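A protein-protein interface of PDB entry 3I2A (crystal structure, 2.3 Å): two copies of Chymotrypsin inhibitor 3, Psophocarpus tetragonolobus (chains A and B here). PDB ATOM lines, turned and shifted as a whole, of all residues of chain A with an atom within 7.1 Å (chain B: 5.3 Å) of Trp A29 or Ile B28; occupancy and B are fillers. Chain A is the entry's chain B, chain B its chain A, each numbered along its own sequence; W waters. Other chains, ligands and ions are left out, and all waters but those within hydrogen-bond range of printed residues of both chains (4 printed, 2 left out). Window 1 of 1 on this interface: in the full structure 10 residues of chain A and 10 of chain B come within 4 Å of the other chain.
OE1 of Glu A55 sits close to OE2 of Glu B173 (2.7 Å).
The side-chain amide nitrogen (ND2) of Asn B170 sits at hydrogen-bond distance from the backbone carbonyl oxygen (O) of His A27 (3.3 Å).
The indole nitrogen (NE1) of Trp B29 lies within hydrogen-bond range of the backbone carbonyl oxygen (O) of Pro A26, at 2.9 Å.
NE1 of Trp A29 sits close to ND2 of Asn B170 (3.0 Å).
The backbone NH of Trp B29 is in hydrogen-bond range of the backbone carbonyl oxygen of Glu A55, at 3.0 Å.
The backbone carbonyl oxygen (O) of Ala B30 is in hydrogen-bond range of the guanidinium group (NH2) of Arg B51 (2.5 Å).
N of His B27 is in hydrogen-bond range of O of Glu B173 (2.7 Å).
N of Val A56 sits close to OD1 of Asn A54, at 3.0 Å.
Among the printed residues, pairs that only touch across the chains: Ile A28 with Asn B170 (3.2 Å), Trp A29 with Trp B29 (3.4 Å), Trp A29 with Ala B30 (3.4 Å), Trp A29 with Ile B28 (3.4 Å), Val A56 with His B27 (3.4 Å), Glu A55 with Ile B28 (3.5 Å), Ala A30 with Glu B173 (3.6 Å), Trp A29 with Pro B171 (3.6 Å), Glu A55 with His B27 (3.9 Å), Gly A32 with Trp B29 (3.9 Å) and Val A56 with Ile B28 (3.97 Å).
Of the printed residues of chain B, Val A56 touches His B27 and Ile B28.
Of the printed residues of chain A, Ile B28 touches Trp A29 (3.4 Å), Glu A55 (3.5 Å) and Val A56 (3.97 Å).
Arg B51 touches none of the printed residues of chain A.
Printed residues of chain A within 4 Å of Asn B170: His A27 (3.3 Å), Ile A28 (3.2 Å) and Trp A29 (3.0 Å).
Leu B172 touches none of the printed residues of chain A.
Printed residues of chain B that touch a printed residue of chain A: His B27, Ile B28, Trp B29, Ala B30, Asn B170, Pro B171 and Glu B173.
Among the printed residues, 16 pairs touch across the chains.
Pro A26 touches Trp B29, but with the chains exchanged Trp A29 does not touch Pro B26 (7.8 Å).
Trp A29 touches Ile B28, but with the chains exchanged Ile A28 does not touch Trp B29 (5.4 Å).
Trp A29 touches its own counterpart, Trp B29.
Trp A29 touches Ala B30, but with the chains exchanged Ala A30 does not touch Trp B29 (6.7 Å).
5 positions are printed for both chains.
Of the 16 pairs that touch across the chains among the printed residues, 1 has its exchanged pair printed and touching as well.
Water W4 lies within hydrogen-bond range of the backbone carbonyl oxygen of Asn B170 (2.5 Å), the backbone NH of Ile B154 (3.0 Å) and the indole nitrogen of Trp A29 (3.3 Å).
Water W1 lies within hydrogen-bond range of O of Val A56 (2.5 Å) and O of Trp B29 (2.6 Å).
Water W3 lies within hydrogen-bond range of the backbone carbonyl oxygen (O) of Pro B171 (2.8 Å), the side-chain amide oxygen (OD1) of Asn B170 (2.8 Å), the backbone NH (N) of Ala A30 (2.9 Å) and the backbone NH (N) of Trp A29 (3.5 Å).
Water W2 lies within hydrogen-bond range of OE2 of Glu A55, NE2 of His B27 and OD1 of Asn A54.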
ATOM      1  N   PRO A  26     -24.585  29.329  30.692  1.00  0.00           N
ATOM      2  CA  PRO A  26     -25.300  28.163  31.207  1.00  0.00           C
ATOM      3  C   PRO A  26     -24.808  26.854  30.623  1.00  0.00           C
ATOM      4  O   PRO A  26     -24.494  26.768  29.443  1.00  0.00           O
ATOM      5  CB  PRO A  26     -26.739  28.451  30.806  1.00  0.00           C
ATOM      6  CG  PRO A  26     -26.542  29.047  29.440  1.00  0.00           C
ATOM      7  CD  PRO A  26     -25.387  30.015  29.661  1.00  0.00           C
ATOM      8  N   HIS A  27     -24.742  25.829  31.460  1.00  0.00           N
ATOM      9  CA  HIS A  27     -24.324  24.520  30.995  1.00  0.00           C
ATOM     10  C   HIS A  27     -25.399  24.045  30.015  1.00  0.00           C
ATOM     11  O   HIS A  27     -25.092  23.467  28.972  1.00  0.00           O
ATOM     12  CB  HIS A  27     -24.209  23.549  32.171  1.00  0.00           C
ATOM     13  CG  HIS A  27     -23.928  22.138  31.758  1.00  0.00           C
ATOM     14  ND1 HIS A  27     -22.875  21.803  30.933  1.00  0.00           N
ATOM     15  CD2 HIS A  27     -24.566  20.979  32.047  1.00  0.00           C
ATOM     16  CE1 HIS A  27     -22.880  20.497  30.729  1.00  0.00           C
ATOM     17  NE2 HIS A  27     -23.896  19.974  31.393  1.00  0.00           N
ATOM     18  N   ILE A  28     -26.655  24.313  30.361  1.00  0.00           N
ATOM     19  CA  ILE A  28     -27.794  23.939  29.527  1.00  0.00           C
ATOM     20  C   ILE A  28     -28.024  25.076  28.526  1.00  0.00           C
ATOM     21  O   ILE A  28     -28.482  26.163  28.899  1.00  0.00           O
ATOM     22  CB  ILE A  28     -29.056  23.737  30.396  1.00  0.00           C
ATOM     23  CG1 ILE A  28     -28.759  22.722  31.511  1.00  0.00           C
ATOM     24  CG2 ILE A  28     -30.223  23.274  29.533  1.00  0.00           C
ATOM     25  CD1 ILE A  28     -28.215  21.368  31.017  1.00  0.00           C
ATOM     26  N   TRP A  29     -27.694  24.815  27.265  1.00  0.00           N
ATOM     27  CA  TRP A  29     -27.816  25.801  26.189  1.00  0.00           C
ATOM     28  C   TRP A  29     -29.150  26.542  26.139  1.00  0.00           C
ATOM     29  O   TRP A  29     -29.186  27.761  25.930  1.00  0.00           O
ATOM     30  CB  TRP A  29     -27.629  25.143  24.817  1.00  0.00           C
ATOM     31  CG  TRP A  29     -26.595  24.076  24.722  1.00  0.00           C
ATOM     32  CD1 TRP A  29     -26.814  22.728  24.641  1.00  0.00           C
ATOM     33  CD2 TRP A  29     -25.182  24.261  24.604  1.00  0.00           C
ATOM     34  NE1 TRP A  29     -25.624  22.061  24.469  1.00  0.00           N
ATOM     35  CE2 TRP A  29     -24.603  22.976  24.445  1.00  0.00           C
ATOM     36  CE3 TRP A  29     -24.344  25.386  24.609  1.00  0.00           C
ATOM     37  CZ2 TRP A  29     -23.221  22.783  24.293  1.00  0.00           C
ATOM     38  CZ3 TRP A  29     -22.965  25.195  24.457  1.00  0.00           C
ATOM     39  CH2 TRP A  29     -22.423  23.897  24.302  1.00  0.00           C
ATOM     40  N   ALA A  30     -30.241  25.795  26.301  1.00  0.00           N
ATOM     41  CA  ALA A  30     -31.585  26.365  26.238  1.00  0.00           C
ATOM     42  C   ALA A  30     -31.871  27.445  27.283  1.00  0.00           C
ATOM     43  O   ALA A  30     -32.804  28.232  27.120  1.00  0.00           O
ATOM     44  CB  ALA A  30     -32.635  25.247  26.346  1.00  0.00           C
ATOM     45  N   HIS A  31     -31.094  27.484  28.359  1.00  0.00           N
ATOM     46  CA  HIS A  31     -31.319  28.505  29.377  1.00  0.00           C
ATOM     47  C   HIS A  31     -31.061  29.911  28.842  1.00  0.00           C
ATOM     48  O   HIS A  31     -31.622  30.873  29.350  1.00  0.00           O
ATOM     49  CB  HIS A  31     -30.439  28.263  30.607  1.00  0.00           C
ATOM     50  CG  HIS A  31     -30.870  27.091  31.428  1.00  0.00           C
ATOM     51  ND1 HIS A  31     -30.304  26.793  32.651  1.00  0.00           N
ATOM     52  CD2 HIS A  31     -31.794  26.131  31.196  1.00  0.00           C
ATOM     53  CE1 HIS A  31     -30.864  25.697  33.133  1.00  0.00           C
ATOM     54  NE2 HIS A  31     -31.770  25.275  32.271  1.00  0.00           N
ATOM     55  N   GLY A  32     -30.214  30.035  27.824  1.00  0.00           N
ATOM     56  CA  GLY A  32     -29.948  31.355  27.283  1.00  0.00           C
ATOM     57  C   GLY A  32     -28.498  31.678  26.987  1.00  0.00           C
ATOM     58  O   GLY A  32     -27.687  30.790  26.709  1.00  0.00           O
ATOM     59  N   GLY A  33     -28.176  32.968  27.039  1.00  0.00           N
ATOM     60  CA  GLY A  33     -26.825  33.411  26.770  1.00  0.00           C
ATOM     61  C   GLY A  33     -26.063  33.830  28.021  1.00  0.00           C
ATOM     62  O   GLY A  33     -26.334  33.345  29.119  1.00  0.00           O
ATOM     63  N   ASN A  54     -30.967  35.635  24.508  1.00  0.00           N
ATOM     64  CA  ASN A  54     -30.394  35.166  23.251  1.00  0.00           C
ATOM     65  C   ASN A  54     -29.367  34.046  23.491  1.00  0.00           C
ATOM     66  O   ASN A  54     -28.215  34.315  23.861  1.00  0.00           O
ATOM     67  CB  ASN A  54     -29.733  36.355  22.543  1.00  0.00           C
ATOM     68  CG  ASN A  54     -29.152  35.990  21.196  1.00  0.00           C
ATOM     69  OD1 ASN A  54     -29.142  34.825  20.803  1.00  0.00           O
ATOM     70  ND2 ASN A  54     -28.655  36.985  20.484  1.00  0.00           N
ATOM     71  N   GLU A  55     -29.792  32.801  23.263  1.00  0.00           N
ATOM     72  CA  GLU A  55     -28.957  31.608  23.458  1.00  0.00           C
ATOM     73  C   GLU A  55     -27.603  31.704  22.784  1.00  0.00           C
ATOM     74  O   GLU A  55     -26.658  31.022  23.166  1.00  0.00           O
ATOM     75  CB  GLU A  55     -29.627  30.351  22.880  1.00  0.00           C
ATOM     76  CG  GLU A  55     -30.981  29.989  23.425  1.00  0.00           C
ATOM     77  CD  GLU A  55     -32.110  30.601  22.623  1.00  0.00           C
ATOM     78  OE1 GLU A  55     -33.160  29.939  22.496  1.00  0.00           O
ATOM     79  OE2 GLU A  55     -31.960  31.739  22.131  1.00  0.00           O
ATOM     80  N   VAL A  56     -27.519  32.534  21.762  1.00  0.00           N
ATOM     81  CA  VAL A  56     -26.296  32.664  20.997  1.00  0.00           C
ATOM     82  C   VAL A  56     -25.314  33.717  21.518  1.00  0.00           C
ATOM     83  O   VAL A  56     -24.147  33.713  21.148  1.00  0.00           O
ATOM     84  CB  VAL A  56     -26.667  32.936  19.503  1.00  0.00           C
ATOM     85  CG1 VAL A  56     -25.475  33.403  18.717  1.00  0.00           C
ATOM     86  CG2 VAL A  56     -27.217  31.658  18.888  1.00  0.00           C
ATOM     87  N   SER A  57     -25.788  34.592  22.398  1.00  0.00           N
ATOM     88  CA  SER A  57     -24.960  35.662  22.941  1.00  0.00           C
ATOM     89  C   SER A  57     -24.154  35.271  24.183  1.00  0.00           C
ATOM     90  O   SER A  57     -24.688  34.674  25.120  1.00  0.00           O
ATOM     91  CB  SER A  57     -25.846  36.867  23.273  1.00  0.00           C
ATOM     92  OG  SER A  57     -25.124  37.830  24.012  1.00  0.00           O
ATOM     93  N   ILE A 131     -15.890  19.026  31.359  1.00  0.00           N
ATOM     94  CA  ILE A 131     -16.183  20.452  31.327  1.00  0.00           C
ATOM     95  C   ILE A 131     -16.721  20.810  32.703  1.00  0.00           C
ATOM     96  O   ILE A 131     -17.716  20.250  33.173  1.00  0.00           O
ATOM     97  CB  ILE A 131     -17.190  20.861  30.229  1.00  0.00           C
ATOM     98  CG1 ILE A 131     -17.331  22.389  30.249  1.00  0.00           C
ATOM     99  CG2 ILE A 131     -18.533  20.177  30.445  1.00  0.00           C
ATOM    100  CD1 ILE A 131     -17.982  22.982  29.022  1.00  0.00           C
ATOM    101  N   ARG A 162     -34.476  38.272  32.854  1.00  0.00           N
ATOM    102  CA  ARG A 162     -34.059  37.111  33.624  1.00  0.00           C
ATOM    103  C   ARG A 162     -33.060  37.585  34.675  1.00  0.00           C
ATOM    104  O   ARG A 162     -31.838  37.502  34.495  1.00  0.00           O
ATOM    105  CB  ARG A 162     -33.440  36.075  32.689  1.00  0.00           C
ATOM    106  CG  ARG A 162     -34.401  35.660  31.595  1.00  0.00           C
ATOM    107  CD  ARG A 162     -33.805  34.667  30.625  1.00  0.00           C
ATOM    108  NE  ARG A 162     -34.724  34.421  29.518  1.00  0.00           N
ATOM    109  CZ  ARG A 162     -34.503  33.554  28.536  1.00  0.00           C
ATOM    110  NH1 ARG A 162     -33.384  32.835  28.518  1.00  0.00           N
ATOM    111  NH2 ARG A 162     -35.397  33.412  27.566  1.00  0.00           N
ATOM    112  N   PRO B  26     -26.525  24.385  14.728  1.00  0.00           N
ATOM    113  CA  PRO B  26     -26.749  24.559  16.168  1.00  0.00           C
ATOM    114  C   PRO B  26     -26.953  26.035  16.537  1.00  0.00           C
ATOM    115  O   PRO B  26     -26.220  26.910  16.087  1.00  0.00           O
ATOM    116  CB  PRO B  26     -25.477  23.982  16.777  1.00  0.00           C
ATOM    117  CG  PRO B  26     -25.181  22.818  15.841  1.00  0.00           C
ATOM    118  CD  PRO B  26     -25.443  23.413  14.463  1.00  0.00           C
ATOM    119  N   HIS B  27     -27.963  26.307  17.355  1.00  0.00           N
ATOM    120  CA  HIS B  27     -28.251  27.670  17.774  1.00  0.00           C
ATOM    121  C   HIS B  27     -28.005  27.702  19.282  1.00  0.00           C
ATOM    122  O   HIS B  27     -28.952  27.706  20.078  1.00  0.00           O
ATOM    123  CB  HIS B  27     -29.710  28.006  17.456  1.00  0.00           C
ATOM    124  CG  HIS B  27     -30.032  29.464  17.539  1.00  0.00           C
ATOM    125  ND1 HIS B  27     -29.635  30.369  16.575  1.00  0.00           N
ATOM    126  CD2 HIS B  27     -30.696  30.180  18.478  1.00  0.00           C
ATOM    127  CE1 HIS B  27     -30.039  31.579  16.919  1.00  0.00           C
ATOM    128  NE2 HIS B  27     -30.683  31.494  18.070  1.00  0.00           N
ATOM    129  N   ILE B  28     -26.726  27.686  19.661  1.00  0.00           N
ATOM    130  CA  ILE B  28     -26.312  27.700  21.066  1.00  0.00           C
ATOM    131  C   ILE B  28     -25.093  28.606  21.222  1.00  0.00           C
ATOM    132  O   ILE B  28     -24.531  29.056  20.219  1.00  0.00           O
ATOM    133  CB  ILE B  28     -25.973  26.280  21.551  1.00  0.00           C
ATOM    134  CG1 ILE B  28     -24.789  25.723  20.754  1.00  0.00           C
ATOM    135  CG2 ILE B  28     -27.199  25.379  21.411  1.00  0.00           C
ATOM    136  CD1 ILE B  28     -24.378  24.316  21.161  1.00  0.00           C
ATOM    137  N   TRP B  29     -24.655  28.866  22.455  1.00  0.00           N
ATOM    138  CA  TRP B  29     -23.540  29.794  22.628  1.00  0.00           C
ATOM    139  C   TRP B  29     -22.157  29.327  22.185  1.00  0.00           C
ATOM    140  O   TRP B  29     -21.324  30.152  21.796  1.00  0.00           O
ATOM    141  CB  TRP B  29     -23.484  30.336  24.069  1.00  0.00           C
ATOM    142  CG  TRP B  29     -23.348  29.316  25.154  1.00  0.00           C
ATOM    143  CD1 TRP B  29     -24.330  28.880  25.997  1.00  0.00           C
ATOM    144  CD2 TRP B  29     -22.152  28.617  25.532  1.00  0.00           C
ATOM    145  NE1 TRP B  29     -23.822  27.954  26.876  1.00  0.00           N
ATOM    146  CE2 TRP B  29     -22.487  27.774  26.613  1.00  0.00           C
ATOM    147  CE3 TRP B  29     -20.827  28.623  25.058  1.00  0.00           C
ATOM    148  CZ2 TRP B  29     -21.549  26.942  27.234  1.00  0.00           C
ATOM    149  CZ3 TRP B  29     -19.894  27.794  25.675  1.00  0.00           C
ATOM    150  CH2 TRP B  29     -20.262  26.964  26.754  1.00  0.00           C
ATOM    151  N   ALA B  30     -21.914  28.022  22.214  1.00  0.00           N
ATOM    152  CA  ALA B  30     -20.616  27.485  21.807  1.00  0.00           C
ATOM    153  C   ALA B  30     -20.391  27.651  20.313  1.00  0.00           C
ATOM    154  O   ALA B  30     -21.264  27.316  19.509  1.00  0.00           O
ATOM    155  CB  ALA B  30     -20.516  26.003  22.179  1.00  0.00           C
ATOM    156  N   ARG B  51     -21.233  17.409  15.339  1.00  0.00           N
ATOM    157  CA  ARG B  51     -21.341  18.816  14.999  1.00  0.00           C
ATOM    158  C   ARG B  51     -19.926  19.262  14.651  1.00  0.00           C
ATOM    159  O   ARG B  51     -18.993  19.036  15.414  1.00  0.00           O
ATOM    160  CB  ARG B  51     -21.886  19.620  16.185  1.00  0.00           C
ATOM    161  CG  ARG B  51     -21.060  20.851  16.563  1.00  0.00           C
ATOM    162  CD  ARG B  51     -21.782  22.172  16.352  1.00  0.00           C
ATOM    163  NE  ARG B  51     -21.583  23.039  17.507  1.00  0.00           N
ATOM    164  CZ  ARG B  51     -21.745  24.359  17.525  1.00  0.00           C
ATOM    165  NH1 ARG B  51     -22.112  25.025  16.437  1.00  0.00           N
ATOM    166  NH2 ARG B  51     -21.537  25.022  18.650  1.00  0.00           N
ATOM    167  N   ILE B 154     -25.398  17.141  22.395  1.00  0.00           N
ATOM    168  CA  ILE B 154     -24.002  16.957  22.012  1.00  0.00           C
ATOM    169  C   ILE B 154     -23.151  16.475  23.174  1.00  0.00           C
ATOM    170  O   ILE B 154     -23.197  17.039  24.269  1.00  0.00           O
ATOM    171  CB  ILE B 154     -23.370  18.273  21.517  1.00  0.00           C
ATOM    172  CG1 ILE B 154     -24.096  18.776  20.273  1.00  0.00           C
ATOM    173  CG2 ILE B 154     -21.898  18.054  21.189  1.00  0.00           C
ATOM    174  CD1 ILE B 154     -23.618  20.143  19.820  1.00  0.00           C
ATOM    175  N   ASN B 170     -29.855  18.207  28.276  1.00  0.00           N
ATOM    176  CA  ASN B 170     -29.310  19.296  27.476  1.00  0.00           C
ATOM    177  C   ASN B 170     -29.528  19.242  25.967  1.00  0.00           C
ATOM    178  O   ASN B 170     -28.610  18.955  25.205  1.00  0.00           O
ATOM    179  CB  ASN B 170     -27.813  19.416  27.777  1.00  0.00           C
ATOM    180  CG  ASN B 170     -27.255  20.755  27.388  1.00  0.00           C
ATOM    181  OD1 ASN B 170     -27.994  21.735  27.283  1.00  0.00           O
ATOM    182  ND2 ASN B 170     -25.939  20.818  27.186  1.00  0.00           N
ATOM    183  N   PRO B 171     -30.750  19.544  25.511  1.00  0.00           N
ATOM    184  CA  PRO B 171     -31.013  19.509  24.074  1.00  0.00           C
ATOM    185  C   PRO B 171     -30.377  20.610  23.252  1.00  0.00           C
ATOM    186  O   PRO B 171     -30.194  21.748  23.697  1.00  0.00           O
ATOM    187  CB  PRO B 171     -32.531  19.581  23.995  1.00  0.00           C
ATOM    188  CG  PRO B 171     -32.878  20.410  25.187  1.00  0.00           C
ATOM    189  CD  PRO B 171     -31.985  19.835  26.265  1.00  0.00           C
ATOM    190  N   LEU B 172     -30.049  20.238  22.027  1.00  0.00           N
ATOM    191  CA  LEU B 172     -29.492  21.148  21.059  1.00  0.00           C
ATOM    192  C   LEU B 172     -30.656  22.010  20.604  1.00  0.00           C
ATOM    193  O   LEU B 172     -31.806  21.615  20.742  1.00  0.00           O
ATOM    194  CB  LEU B 172     -29.025  20.372  19.827  1.00  0.00           C
ATOM    195  CG  LEU B 172     -27.574  19.983  19.613  1.00  0.00           C
ATOM    196  CD1 LEU B 172     -27.460  19.199  18.304  1.00  0.00           C
ATOM    197  CD2 LEU B 172     -26.718  21.246  19.573  1.00  0.00           C
ATOM    198  N   GLU B 173     -30.348  23.185  20.067  1.00  0.00           N
ATOM    199  CA  GLU B 173     -31.357  24.032  19.462  1.00  0.00           C
ATOM    200  C   GLU B 173     -30.743  24.182  18.081  1.00  0.00           C
ATOM    201  O   GLU B 173     -29.519  24.221  17.964  1.00  0.00           O
ATOM    202  CB  GLU B 173     -31.475  25.381  20.156  1.00  0.00           C
ATOM    203  CG  GLU B 173     -32.187  25.292  21.483  1.00  0.00           C
ATOM    204  CD  GLU B 173     -32.651  26.646  21.969  1.00  0.00           C
ATOM    205  OE1 GLU B 173     -33.226  26.702  23.072  1.00  0.00           O
ATOM    206  OE2 GLU B 173     -32.447  27.648  21.245  1.00  0.00           O
HETATM  207  O   HOH W   1     -22.455  31.977  20.410  1.00  0.00           O
HETATM  208  O   HOH W   2     -31.928  33.520  19.930  1.00  0.00           O
HETATM  209  O   HOH W   3     -30.401  22.867  26.282  1.00  0.00           O
HETATM  210  O   HOH W   4     -26.138  18.792  24.840  1.00  0.00           O
